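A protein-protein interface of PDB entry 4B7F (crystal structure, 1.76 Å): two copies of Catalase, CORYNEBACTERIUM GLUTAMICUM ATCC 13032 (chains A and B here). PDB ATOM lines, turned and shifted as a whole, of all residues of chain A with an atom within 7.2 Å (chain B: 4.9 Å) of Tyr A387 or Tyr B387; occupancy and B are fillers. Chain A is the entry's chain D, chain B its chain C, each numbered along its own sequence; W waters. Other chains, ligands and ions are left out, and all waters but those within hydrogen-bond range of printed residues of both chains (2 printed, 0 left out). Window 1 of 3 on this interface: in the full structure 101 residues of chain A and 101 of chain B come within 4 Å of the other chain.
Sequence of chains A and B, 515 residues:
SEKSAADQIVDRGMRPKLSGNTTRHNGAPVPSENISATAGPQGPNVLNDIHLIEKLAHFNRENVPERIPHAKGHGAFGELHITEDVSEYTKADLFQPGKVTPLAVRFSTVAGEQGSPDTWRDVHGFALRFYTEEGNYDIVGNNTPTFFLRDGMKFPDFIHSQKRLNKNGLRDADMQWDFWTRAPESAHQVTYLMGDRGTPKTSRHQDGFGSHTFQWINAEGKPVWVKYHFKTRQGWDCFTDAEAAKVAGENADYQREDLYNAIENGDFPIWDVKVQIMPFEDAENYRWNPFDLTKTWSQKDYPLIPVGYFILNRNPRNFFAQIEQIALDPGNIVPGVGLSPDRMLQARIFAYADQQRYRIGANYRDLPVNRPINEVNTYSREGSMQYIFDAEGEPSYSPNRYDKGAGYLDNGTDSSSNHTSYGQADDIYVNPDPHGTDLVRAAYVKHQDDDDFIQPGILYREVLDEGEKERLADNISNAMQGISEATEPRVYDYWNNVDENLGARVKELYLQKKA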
ATOM      1  N   ARG A  12       9.019  13.661   9.950  1.00  0.00           N
ATOM      2  CA  ARG A  12      10.261  13.071   9.436  1.00  0.00           C
ATOM      3  C   ARG A  12      10.235  11.550   9.514  1.00  0.00           C
ATOM      4  O   ARG A  12       9.961  10.989  10.583  1.00  0.00           O
ATOM      5  CB  ARG A  12      11.461  13.525  10.260  1.00  0.00           C
ATOM      6  CG  ARG A  12      11.808  14.985  10.203  1.00  0.00           C
ATOM      7  CD  ARG A  12      12.905  15.245  11.215  1.00  0.00           C
ATOM      8  NE  ARG A  12      13.438  16.601  11.135  1.00  0.00           N
ATOM      9  CZ  ARG A  12      14.300  17.103  12.008  1.00  0.00           C
ATOM     10  NH1 ARG A  12      14.724  16.353  13.014  1.00  0.00           N
ATOM     11  NH2 ARG A  12      14.740  18.343  11.879  1.00  0.00           N
ATOM     12  N   GLY A  13      10.536  10.888   8.394  1.00  0.00           N
ATOM     13  CA  GLY A  13      10.659   9.439   8.370  1.00  0.00           C
ATOM     14  C   GLY A  13       9.366   8.682   8.143  1.00  0.00           C
ATOM     15  O   GLY A  13       9.382   7.459   8.013  1.00  0.00           O
ATOM     16  N   MET A  14       8.242   9.393   8.085  1.00  0.00           N
ATOM     17  CA  MET A  14       6.952   8.727   7.982  1.00  0.00           C
ATOM     18  C   MET A  14       6.582   8.413   6.531  1.00  0.00           C
ATOM     19  O   MET A  14       6.619   9.296   5.666  1.00  0.00           O
ATOM     20  CB  MET A  14       5.848   9.576   8.617  1.00  0.00           C
ATOM     21  CG  MET A  14       4.495   8.881   8.613  1.00  0.00           C
ATOM     22  SD  MET A  14       3.298   9.653   9.729  1.00  0.00           S
ATOM     23  CE  MET A  14       3.305  11.343   9.149  1.00  0.00           C
ATOM     24  N   ALA A 321       9.286   4.695  17.357  1.00  0.00           N
ATOM     25  CA  ALA A 321      10.261   5.401  16.532  1.00  0.00           C
ATOM     26  C   ALA A 321      10.616   6.761  17.093  1.00  0.00           C
ATOM     27  O   ALA A 321      11.749   7.233  16.938  1.00  0.00           O
ATOM     28  CB  ALA A 321       9.759   5.527  15.099  1.00  0.00           C
ATOM     29  N   GLN A 325      12.930   5.611  20.896  1.00  0.00           N
ATOM     30  CA  GLN A 325      14.206   5.985  20.274  1.00  0.00           C
ATOM     31  C   GLN A 325      14.688   7.420  20.503  1.00  0.00           C
ATOM     32  O   GLN A 325      15.802   7.769  20.108  1.00  0.00           O
ATOM     33  CB  GLN A 325      14.152   5.718  18.769  1.00  0.00           C
ATOM     34  CG  GLN A 325      13.993   4.258  18.434  1.00  0.00           C
ATOM     35  CD  GLN A 325      14.208   3.987  16.972  1.00  0.00           C
ATOM     36  OE1 GLN A 325      14.832   2.985  16.599  1.00  0.00           O
ATOM     37  NE2 GLN A 325      13.699   4.882  16.123  1.00  0.00           N
ATOM     38  N   ASN A 363      25.023   5.634  15.545  1.00  0.00           N
ATOM     39  CA  ASN A 363      24.473   6.708  14.729  1.00  0.00           C
ATOM     40  C   ASN A 363      23.094   7.188  15.173  1.00  0.00           C
ATOM     41  O   ASN A 363      22.333   7.751  14.380  1.00  0.00           O
ATOM     42  CB  ASN A 363      24.501   6.309  13.247  1.00  0.00           C
ATOM     43  CG  ASN A 363      25.888   6.470  12.652  1.00  0.00           C
ATOM     44  OD1 ASN A 363      26.555   7.477  12.909  1.00  0.00           O
ATOM     45  ND2 ASN A 363      26.349   5.470  11.900  1.00  0.00           N
ATOM     46  N   TYR A 364      22.802   7.002  16.459  1.00  0.00           N
ATOM     47  CA  TYR A 364      21.497   7.350  17.030  1.00  0.00           C
ATOM     48  C   TYR A 364      21.116   8.820  16.793  1.00  0.00           C
ATOM     49  O   TYR A 364      19.927   9.169  16.773  1.00  0.00           O
ATOM     50  CB  TYR A 364      21.485   7.042  18.542  1.00  0.00           C
ATOM     51  CG  TYR A 364      22.287   8.010  19.398  1.00  0.00           C
ATOM     52  CD1 TYR A 364      23.648   7.814  19.629  1.00  0.00           C
ATOM     53  CD2 TYR A 364      21.672   9.105  20.002  1.00  0.00           C
ATOM     54  CE1 TYR A 364      24.378   8.696  20.416  1.00  0.00           C
ATOM     55  CE2 TYR A 364      22.401  10.002  20.786  1.00  0.00           C
ATOM     56  CZ  TYR A 364      23.748   9.791  20.990  1.00  0.00           C
ATOM     57  OH  TYR A 364      24.458  10.682  21.777  1.00  0.00           O
ATOM     58  N   ARG A 365      22.123   9.673  16.618  1.00  0.00           N
ATOM     59  CA  ARG A 365      21.892  11.110  16.450  1.00  0.00           C
ATOM     60  C   ARG A 365      21.239  11.422  15.111  1.00  0.00           C
ATOM     61  O   ARG A 365      20.661  12.496  14.933  1.00  0.00           O
ATOM     62  CB  ARG A 365      23.215  11.873  16.522  1.00  0.00           C
ATOM     63  CG  ARG A 365      23.893  11.839  17.885  1.00  0.00           C
ATOM     64  CD  ARG A 365      23.435  12.984  18.776  1.00  0.00           C
ATOM     65  NE  ARG A 365      24.288  13.117  19.950  1.00  0.00           N
ATOM     66  CZ  ARG A 365      24.158  14.066  20.874  1.00  0.00           C
ATOM     67  NH1 ARG A 365      23.196  14.973  20.765  1.00  0.00           N
ATOM     68  NH2 ARG A 365      24.994  14.106  21.909  1.00  0.00           N
ATOM     69  N   ASP A 366      21.343  10.491  14.167  1.00  0.00           N
ATOM     70  CA  ASP A 366      20.802  10.709  12.831  1.00  0.00           C
ATOM     71  C   ASP A 366      19.328  10.322  12.691  1.00  0.00           C
ATOM     72  O   ASP A 366      18.704  10.614  11.667  1.00  0.00           O
ATOM     73  CB  ASP A 366      21.652   9.961  11.799  1.00  0.00           C
ATOM     74  CG  ASP A 366      23.090  10.447  11.775  1.00  0.00           C
ATOM     75  OD1 ASP A 366      23.312  11.663  11.974  1.00  0.00           O
ATOM     76  OD2 ASP A 366      24.003   9.619  11.581  1.00  0.00           O
ATOM     77  N   LEU A 367      18.760   9.660  13.701  1.00  0.00           N
ATOM     78  CA  LEU A 367      17.350   9.291  13.620  1.00  0.00           C
ATOM     79  C   LEU A 367      16.502  10.562  13.613  1.00  0.00           C
ATOM     80  O   LEU A 367      16.866  11.533  14.261  1.00  0.00           O
ATOM     81  CB  LEU A 367      16.932   8.397  14.792  1.00  0.00           C
ATOM     82  CG  LEU A 367      17.592   7.026  14.855  1.00  0.00           C
ATOM     83  CD1 LEU A 367      17.286   6.346  16.185  1.00  0.00           C
ATOM     84  CD2 LEU A 367      17.139   6.144  13.683  1.00  0.00           C
ATOM     85  N   PRO A 368      15.376  10.551  12.872  1.00  0.00           N
ATOM     86  CA  PRO A 368      14.499  11.720  12.719  1.00  0.00           C
ATOM     87  C   PRO A 368      14.281  12.513  14.013  1.00  0.00           C
ATOM     88  O   PRO A 368      14.517  13.717  14.019  1.00  0.00           O
ATOM     89  CB  PRO A 368      13.200  11.099  12.221  1.00  0.00           C
ATOM     90  CG  PRO A 368      13.681   9.981  11.327  1.00  0.00           C
ATOM     91  CD  PRO A 368      14.933   9.430  12.018  1.00  0.00           C
ATOM     92  N   ARG A 371      17.642  14.447  15.347  1.00  0.00           N
ATOM     93  CA  ARG A 371      18.322  15.425  14.524  1.00  0.00           C
ATOM     94  C   ARG A 371      17.821  16.830  14.821  1.00  0.00           C
ATOM     95  O   ARG A 371      16.621  17.035  15.026  1.00  0.00           O
ATOM     96  CB  ARG A 371      18.101  15.129  13.042  1.00  0.00           C
ATOM     97  CG  ARG A 371      18.786  13.877  12.554  1.00  0.00           C
ATOM     98  CD  ARG A 371      19.068  13.999  11.067  1.00  0.00           C
ATOM     99  NE  ARG A 371      17.897  14.453  10.319  1.00  0.00           N
ATOM    100  CZ  ARG A 371      16.932  13.645   9.889  1.00  0.00           C
ATOM    101  NH1 ARG A 371      16.995  12.336  10.130  1.00  0.00           N
ATOM    102  NH2 ARG A 371      15.908  14.138   9.208  1.00  0.00           N
ATOM    103  N   GLU A 382      31.036   7.087   9.265  1.00  0.00           N
ATOM    104  CA  GLU A 382      30.877   5.622   9.315  1.00  0.00           C
ATOM    105  C   GLU A 382      30.049   5.131  10.508  1.00  0.00           C
ATOM    106  O   GLU A 382      29.075   5.787  10.897  1.00  0.00           O
ATOM    107  CB  GLU A 382      32.248   4.945   9.166  1.00  0.00           C
ATOM    108  CG  GLU A 382      32.889   5.454   7.864  1.00  0.00           C
ATOM    109  CD  GLU A 382      34.239   4.867   7.517  1.00  0.00           C
ATOM    110  OE1 GLU A 382      34.727   3.970   8.230  1.00  0.00           O
ATOM    111  OE2 GLU A 382      34.812   5.315   6.498  1.00  0.00           O
ATOM    112  N   GLY A 383      30.398   3.977  11.064  1.00  0.00           N
ATOM    113  CA  GLY A 383      29.609   3.413  12.144  1.00  0.00           C
ATOM    114  C   GLY A 383      28.389   2.676  11.622  1.00  0.00           C
ATOM    115  O   GLY A 383      27.917   2.928  10.507  1.00  0.00           O
ATOM    116  N   SER A 384      27.875   1.761  12.435  1.00  0.00           N
ATOM    117  CA  SER A 384      26.717   0.959  12.061  1.00  0.00           C
ATOM    118  C   SER A 384      25.557   1.827  11.588  1.00  0.00           C
ATOM    119  O   SER A 384      25.293   2.887  12.159  1.00  0.00           O
ATOM    120  CB  SER A 384      26.261   0.105  13.251  1.00  0.00           C
ATOM    121  OG  SER A 384      27.307  -0.744  13.689  1.00  0.00           O
ATOM    122  N   MET A 385      24.874   1.369  10.541  1.00  0.00           N
ATOM    123  CA  MET A 385      23.643   2.003  10.076  1.00  0.00           C
ATOM    124  C   MET A 385      23.799   3.502   9.823  1.00  0.00           C
ATOM    125  O   MET A 385      23.015   4.308  10.334  1.00  0.00           O
ATOM    126  CB  MET A 385      22.521   1.752  11.096  1.00  0.00           C
ATOM    127  CG  MET A 385      22.029   0.290  11.146  1.00  0.00           C
ATOM    128  SD  MET A 385      21.010  -0.146   9.709  1.00  0.00           S
ATOM    129  CE  MET A 385      19.512   0.775  10.101  1.00  0.00           C
ATOM    130  N   GLN A 386      24.823   3.879   9.062  1.00  0.00           N
ATOM    131  CA  GLN A 386      24.980   5.272   8.664  1.00  0.00           C
ATOM    132  C   GLN A 386      24.015   5.608   7.525  1.00  0.00           C
ATOM    133  O   GLN A 386      24.192   5.136   6.403  1.00  0.00           O
ATOM    134  CB  GLN A 386      26.417   5.572   8.214  1.00  0.00           C
ATOM    135  CG  GLN A 386      26.576   7.038   7.812  1.00  0.00           C
ATOM    136  CD  GLN A 386      27.947   7.416   7.295  1.00  0.00           C
ATOM    137  OE1 GLN A 386      28.743   6.565   6.896  1.00  0.00           O
ATOM    138  NE2 GLN A 386      28.226   8.717   7.288  1.00  0.00           N
ATOM    139  N   TYR A 387      22.982   6.399   7.807  1.00  0.00           N
ATOM    140  CA  TYR A 387      22.020   6.797   6.779  1.00  0.00           C
ATOM    141  C   TYR A 387      22.498   8.074   6.109  1.00  0.00           C
ATOM    142  O   TYR A 387      22.476   8.201   4.881  1.00  0.00           O
ATOM    143  CB  TYR A 387      20.648   7.053   7.406  1.00  0.00           C
ATOM    144  CG  TYR A 387      19.530   7.336   6.415  1.00  0.00           C
ATOM    145  CD1 TYR A 387      19.494   8.521   5.673  1.00  0.00           C
ATOM    146  CD2 TYR A 387      18.491   6.428   6.244  1.00  0.00           C
ATOM    147  CE1 TYR A 387      18.475   8.778   4.783  1.00  0.00           C
ATOM    148  CE2 TYR A 387      17.466   6.681   5.356  1.00  0.00           C
ATOM    149  CZ  TYR A 387      17.464   7.845   4.632  1.00  0.00           C
ATOM    150  OH  TYR A 387      16.427   8.071   3.758  1.00  0.00           O
ATOM    151  N   ILE A 388      22.917   9.025   6.934  1.00  0.00           N
ATOM    152  CA  ILE A 388      23.300  10.340   6.431  1.00  0.00           C
ATOM    153  C   ILE A 388      24.811  10.448   6.291  1.00  0.00           C
ATOM    154  O   ILE A 388      25.551  10.063   7.192  1.00  0.00           O
ATOM    155  CB  ILE A 388      22.748  11.445   7.367  1.00  0.00           C
ATOM    156  CG1 ILE A 388      21.218  11.377   7.382  1.00  0.00           C
ATOM    157  CG2 ILE A 388      23.239  12.811   6.948  1.00  0.00           C
ATOM    158  CD1 ILE A 388      20.603  12.135   8.521  1.00  0.00           C
ATOM    159  N   PHE A 389      25.275  10.957   5.153  1.00  0.00           N
ATOM    160  CA  PHE A 389      26.711  11.127   4.939  1.00  0.00           C
ATOM    161  C   PHE A 389      27.015  12.504   4.328  1.00  0.00           C
ATOM    162  O   PHE A 389      26.139  13.111   3.703  1.00  0.00           O
ATOM    163  CB  PHE A 389      27.266   9.999   4.055  1.00  0.00           C
ATOM    164  CG  PHE A 389      26.548   9.847   2.742  1.00  0.00           C
ATOM    165  CD1 PHE A 389      25.442   9.013   2.633  1.00  0.00           C
ATOM    166  CD2 PHE A 389      26.982  10.531   1.620  1.00  0.00           C
ATOM    167  CE1 PHE A 389      24.776   8.868   1.427  1.00  0.00           C
ATOM    168  CE2 PHE A 389      26.325  10.401   0.410  1.00  0.00           C
ATOM    169  CZ  PHE A 389      25.209   9.552   0.313  1.00  0.00           C
ATOM    170  N   GLY B  13      20.385  10.470   1.066  1.00  0.00           N
ATOM    171  CA  GLY B  13      21.152  10.504   2.295  1.00  0.00           C
ATOM    172  C   GLY B  13      22.276  11.522   2.348  1.00  0.00           C
ATOM    173  O   GLY B  13      22.878  11.718   3.406  1.00  0.00           O
ATOM    174  N   ASP B 366      16.476  -0.336   5.259  1.00  0.00           N
ATOM    175  CA  ASP B 366      16.015   1.044   5.170  1.00  0.00           C
ATOM    176  C   ASP B 366      17.118   2.024   4.781  1.00  0.00           C
ATOM    177  O   ASP B 366      16.834   3.183   4.479  1.00  0.00           O
ATOM    178  CB  ASP B 366      15.345   1.482   6.475  1.00  0.00           C
ATOM    179  CG  ASP B 366      14.130   0.644   6.814  1.00  0.00           C
ATOM    180  OD1 ASP B 366      13.389   0.250   5.887  1.00  0.00           O
ATOM    181  OD2 ASP B 366      13.914   0.377   8.007  1.00  0.00           O
ATOM    182  N   LEU B 367      18.370   1.566   4.785  1.00  0.00           N
ATOM    183  CA  LEU B 367      19.486   2.416   4.360  1.00  0.00           C
ATOM    184  C   LEU B 367      19.284   2.807   2.890  1.00  0.00           C
ATOM    185  O   LEU B 367      18.819   1.993   2.093  1.00  0.00           O
ATOM    186  CB  LEU B 367      20.826   1.682   4.515  1.00  0.00           C
ATOM    187  CG  LEU B 367      21.461   1.327   5.863  1.00  0.00           C
ATOM    188  CD1 LEU B 367      22.346   0.133   5.725  1.00  0.00           C
ATOM    189  CD2 LEU B 367      22.365   2.453   6.297  1.00  0.00           C
ATOM    190  N   PRO B 368      19.630   4.054   2.532  1.00  0.00           N
ATOM    191  CA  PRO B 368      19.450   4.583   1.175  1.00  0.00           C
ATOM    192  C   PRO B 368      19.803   3.609   0.046  1.00  0.00           C
ATOM    193  O   PRO B 368      18.976   3.424  -0.855  1.00  0.00           O
ATOM    194  CB  PRO B 368      20.389   5.787   1.169  1.00  0.00           C
ATOM    195  CG  PRO B 368      20.234   6.331   2.561  1.00  0.00           C
ATOM    196  CD  PRO B 368      20.176   5.080   3.442  1.00  0.00           C
ATOM    197  N   ARG B 371      17.142   0.515  -0.095  1.00  0.00           N
ATOM    198  CA  ARG B 371      15.702   0.671  -0.343  1.00  0.00           C
ATOM    199  C   ARG B 371      15.407   0.575  -1.827  1.00  0.00           C
ATOM    200  O   ARG B 371      16.180   1.059  -2.644  1.00  0.00           O
ATOM    201  CB  ARG B 371      15.191   2.033   0.140  1.00  0.00           C
ATOM    202  CG  ARG B 371      15.228   2.233   1.629  1.00  0.00           C
ATOM    203  CD  ARG B 371      14.276   3.352   2.041  1.00  0.00           C
ATOM    204  NE  ARG B 371      14.544   4.632   1.368  1.00  0.00           N
ATOM    205  CZ  ARG B 371      15.465   5.512   1.759  1.00  0.00           C
ATOM    206  NH1 ARG B 371      16.237   5.262   2.812  1.00  0.00           N
ATOM    207  NH2 ARG B 371      15.622   6.651   1.093  1.00  0.00           N
ATOM    208  N   MET B 385      17.586   1.299  15.485  1.00  0.00           N
ATOM    209  CA  MET B 385      17.781   2.337  14.474  1.00  0.00           C
ATOM    210  C   MET B 385      16.687   2.338  13.414  1.00  0.00           C
ATOM    211  O   MET B 385      16.973   2.308  12.211  1.00  0.00           O
ATOM    212  CB  MET B 385      19.150   2.149  13.807  1.00  0.00           C
ATOM    213  CG  MET B 385      20.320   2.451  14.743  1.00  0.00           C
ATOM    214  SD  MET B 385      20.479   4.231  15.110  1.00  0.00           S
ATOM    215  CE  MET B 385      21.025   4.845  13.529  1.00  0.00           C
ATOM    216  N   GLN B 386      15.434   2.367  13.852  1.00  0.00           N
ATOM    217  CA  GLN B 386      14.333   2.478  12.912  1.00  0.00           C
ATOM    218  C   GLN B 386      14.223   3.918  12.437  1.00  0.00           C
ATOM    219  O   GLN B 386      13.841   4.809  13.206  1.00  0.00           O
ATOM    220  CB  GLN B 386      13.002   2.056  13.534  1.00  0.00           C
ATOM    221  CG  GLN B 386      11.859   2.195  12.525  1.00  0.00           C
ATOM    222  CD  GLN B 386      10.509   1.769  13.063  1.00  0.00           C
ATOM    223  OE1 GLN B 386      10.307   1.685  14.276  1.00  0.00           O
ATOM    224  NE2 GLN B 386       9.567   1.507  12.155  1.00  0.00           N
ATOM    225  N   TYR B 387      14.567   4.139  11.175  1.00  0.00           N
ATOM    226  CA  TYR B 387      14.538   5.475  10.582  1.00  0.00           C
ATOM    227  C   TYR B 387      13.179   5.752   9.949  1.00  0.00           C
ATOM    228  O   TYR B 387      12.660   6.872  10.010  1.00  0.00           O
ATOM    229  CB  TYR B 387      15.581   5.560   9.475  1.00  0.00           C
ATOM    230  CG  TYR B 387      17.019   5.786   9.898  1.00  0.00           C
ATOM    231  CD1 TYR B 387      17.819   4.727  10.321  1.00  0.00           C
ATOM    232  CD2 TYR B 387      17.593   7.053   9.827  1.00  0.00           C
ATOM    233  CE1 TYR B 387      19.142   4.928  10.692  1.00  0.00           C
ATOM    234  CE2 TYR B 387      18.917   7.266  10.201  1.00  0.00           C
ATOM    235  CZ  TYR B 387      19.694   6.198  10.614  1.00  0.00           C
ATOM    236  OH  TYR B 387      21.020   6.401  10.957  1.00  0.00           O
ATOM    237  N   ILE B 388      12.625   4.723   9.314  1.00  0.00           N
ATOM    238  CA  ILE B 388      11.412   4.864   8.523  1.00  0.00           C
ATOM    239  C   ILE B 388      10.281   4.122   9.219  1.00  0.00           C
ATOM    240  O   ILE B 388      10.469   2.988   9.666  1.00  0.00           O
ATOM    241  CB  ILE B 388      11.629   4.287   7.103  1.00  0.00           C
ATOM    242  CG1 ILE B 388      12.735   5.059   6.392  1.00  0.00           C
ATOM    243  CG2 ILE B 388      10.340   4.334   6.291  1.00  0.00           C
ATOM    244  CD1 ILE B 388      13.113   4.487   5.044  1.00  0.00           C
ATOM    245  N   PHE B 389       9.111   4.759   9.315  1.00  0.00           N
ATOM    246  CA  PHE B 389       7.941   4.131   9.929  1.00  0.00           C
ATOM    247  C   PHE B 389       6.660   4.374   9.117  1.00  0.00           C
ATOM    248  O   PHE B 389       6.579   5.325   8.325  1.00  0.00           O
ATOM    249  CB  PHE B 389       7.762   4.585  11.395  1.00  0.00           C
ATOM    250  CG  PHE B 389       7.720   6.084  11.573  1.00  0.00           C
ATOM    251  CD1 PHE B 389       6.516   6.776  11.497  1.00  0.00           C
ATOM    252  CD2 PHE B 389       8.880   6.795  11.839  1.00  0.00           C
ATOM    253  CE1 PHE B 389       6.478   8.151  11.668  1.00  0.00           C
ATOM    254  CE2 PHE B 389       8.858   8.172  12.004  1.00  0.00           C
ATOM    255  CZ  PHE B 389       7.654   8.855  11.922  1.00  0.00           C
HETATM  256  O   HOH W   1      23.148   8.217   9.676  1.00  0.00           O
HETATM  257  O   HOH W   2      16.692   1.781  18.174  1.00  0.00           O
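N of Phe A389 is in hydrogen-bond range of O of Gly B13 (3.1 Å). The side-chain hydroxyl of Tyr A387 sits at hydrogen-bond distance from the guanidinium group of Arg B371. N of Met B385 is in hydrogen-bond range of OE1 of Gln A325 (3.4 Å). The side-chain amide oxygen (OE1) of Gln A325 lies within hydrogen-bond range of the backbone NH (N) of Gln B386 (2.9 Å). OH of Tyr B387 is in hydrogen-bond range of O of Met A385 (3.0 Å). The backbone carbonyl oxygen (O) of Gly A13 lies within hydrogen-bond range of the backbone NH (N) of Phe B389, 3.0 Å away.
The backbone carbonyl oxygen of Asp B366 is in hydrogen-bond range of the guanidinium group of Arg B371 (2.7 Å). NH1 of Arg A12 is in hydrogen-bond range of O of Arg A371 (2.8 Å). ND2 of Asn A363 sits at hydrogen-bond distance from O of Glu A382 (2.9 Å). ND2 of Asn A363 sits at hydrogen-bond distance from O of Gly A383 (3.3 Å). ND2 of Asn A363 lies within hydrogen-bond range of O of Ser A384. N of Glu A382 is in hydrogen-bond range of OE1 of Gln A386, at 3.3 Å.
Phe B389 touches Arg A12. O of Tyr B387 touches CA of Gly A13 (3.6 Å). O of Gly A13 touches CA of Ile B388 (3.3 Å). Tyr B387 touches Asn A363. Tyr B387 touches Asp A366 (CE2 to O, 3.7 Å). Gln B386 touches Leu A367 (O to CD2, 3.6 Å). Leu B367 touches Met A385 (CD2 to C, 3.9 Å). Met A385 touches Met B385 (CE to O, 3.6 Å). Gln A386 touches Leu B367. Tyr A387 touches Tyr B387.
Of the printed residues of chain B, Tyr A387 touches Gly B13, Asp B366, Pro B368, Arg B371 and Tyr B387. Of the printed residues of chain A, Tyr B387 touches Gly A13 (3.6 Å), Asn A363 (3.9 Å), Asp A366 (3.7 Å), Leu A367 (3.7 Å), Pro A368 (3.5 Å), Met A385 (3.0 Å) and Tyr A387 (3.3 Å). Of the printed residues of chain B, Met A14 touches Phe B389. Of the printed residues of chain B, Gly A13 touches Tyr B387, Ile B388 and Phe B389. Of the printed residues of chain B, Phe A389 touches Gly B13. Of the printed residues of chain A, Leu B367 touches Met A385 and Gln A386. Printed residues of chain A within 4 Å of Pro B368: Tyr A387 (3.5 Å). Glu A382 touches none of the printed residues of chain B.
Printed residues of chain B that touch a printed residue of chain A: Gly B13, Asp B366, Leu B367, Pro B368, Arg B371, Met B385, Gln B386, Tyr B387, Ile B388 and Phe B389. Hydrophobic or aromatic side chains of chain B that line the printed part of chain A: Leu B367, Pro B368, Met B385, Tyr B387, Ile B388 and Phe B389. Of the 20 printed residues of chain A, 15 touch a printed residue of chain B. Printed residues of chain A that touch a printed residue of chain B: Arg A12, Gly A13, Met A14, Ala A321, Gln A325, Asn A363, Tyr A364, Asp A366, Leu A367, Pro A368, Met A385, Gln A386, Tyr A387, Ile A388 and Phe A389. Along chain A the printed residues that touch a printed residue of chain B span positions 12 to 389.
Leu A367 touches Gln B386, and with the chains exchanged Gln A386 touches Leu B367. Met B385 touches its own counterpart, Met A385. Tyr A387 touches Arg B371, but with the chains exchanged Arg A371 does not touch Tyr B387 (5.3 Å). Tyr B387 touches its own counterpart, Tyr A387. Positions printed for both chains: 13, 366, 367, 368, 371, 385, 386, 387, 388 and 389.
Water W1 lies within hydrogen-bond range of the side-chain carboxylate (OD2) of Asp A366 (2.5 Å), the backbone NH (N) of Tyr A387 (2.6 Å), the backbone NH (N) of Ile A388 (2.9 Å) and the side-chain hydroxyl (OH) of Tyr B387 (3.1 Å). Water W2 bridges the side-chain amide oxygen (OE1) of Gln A325 (2.7 Å) and the backbone NH (N) of Met B385 (2.9 Å).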
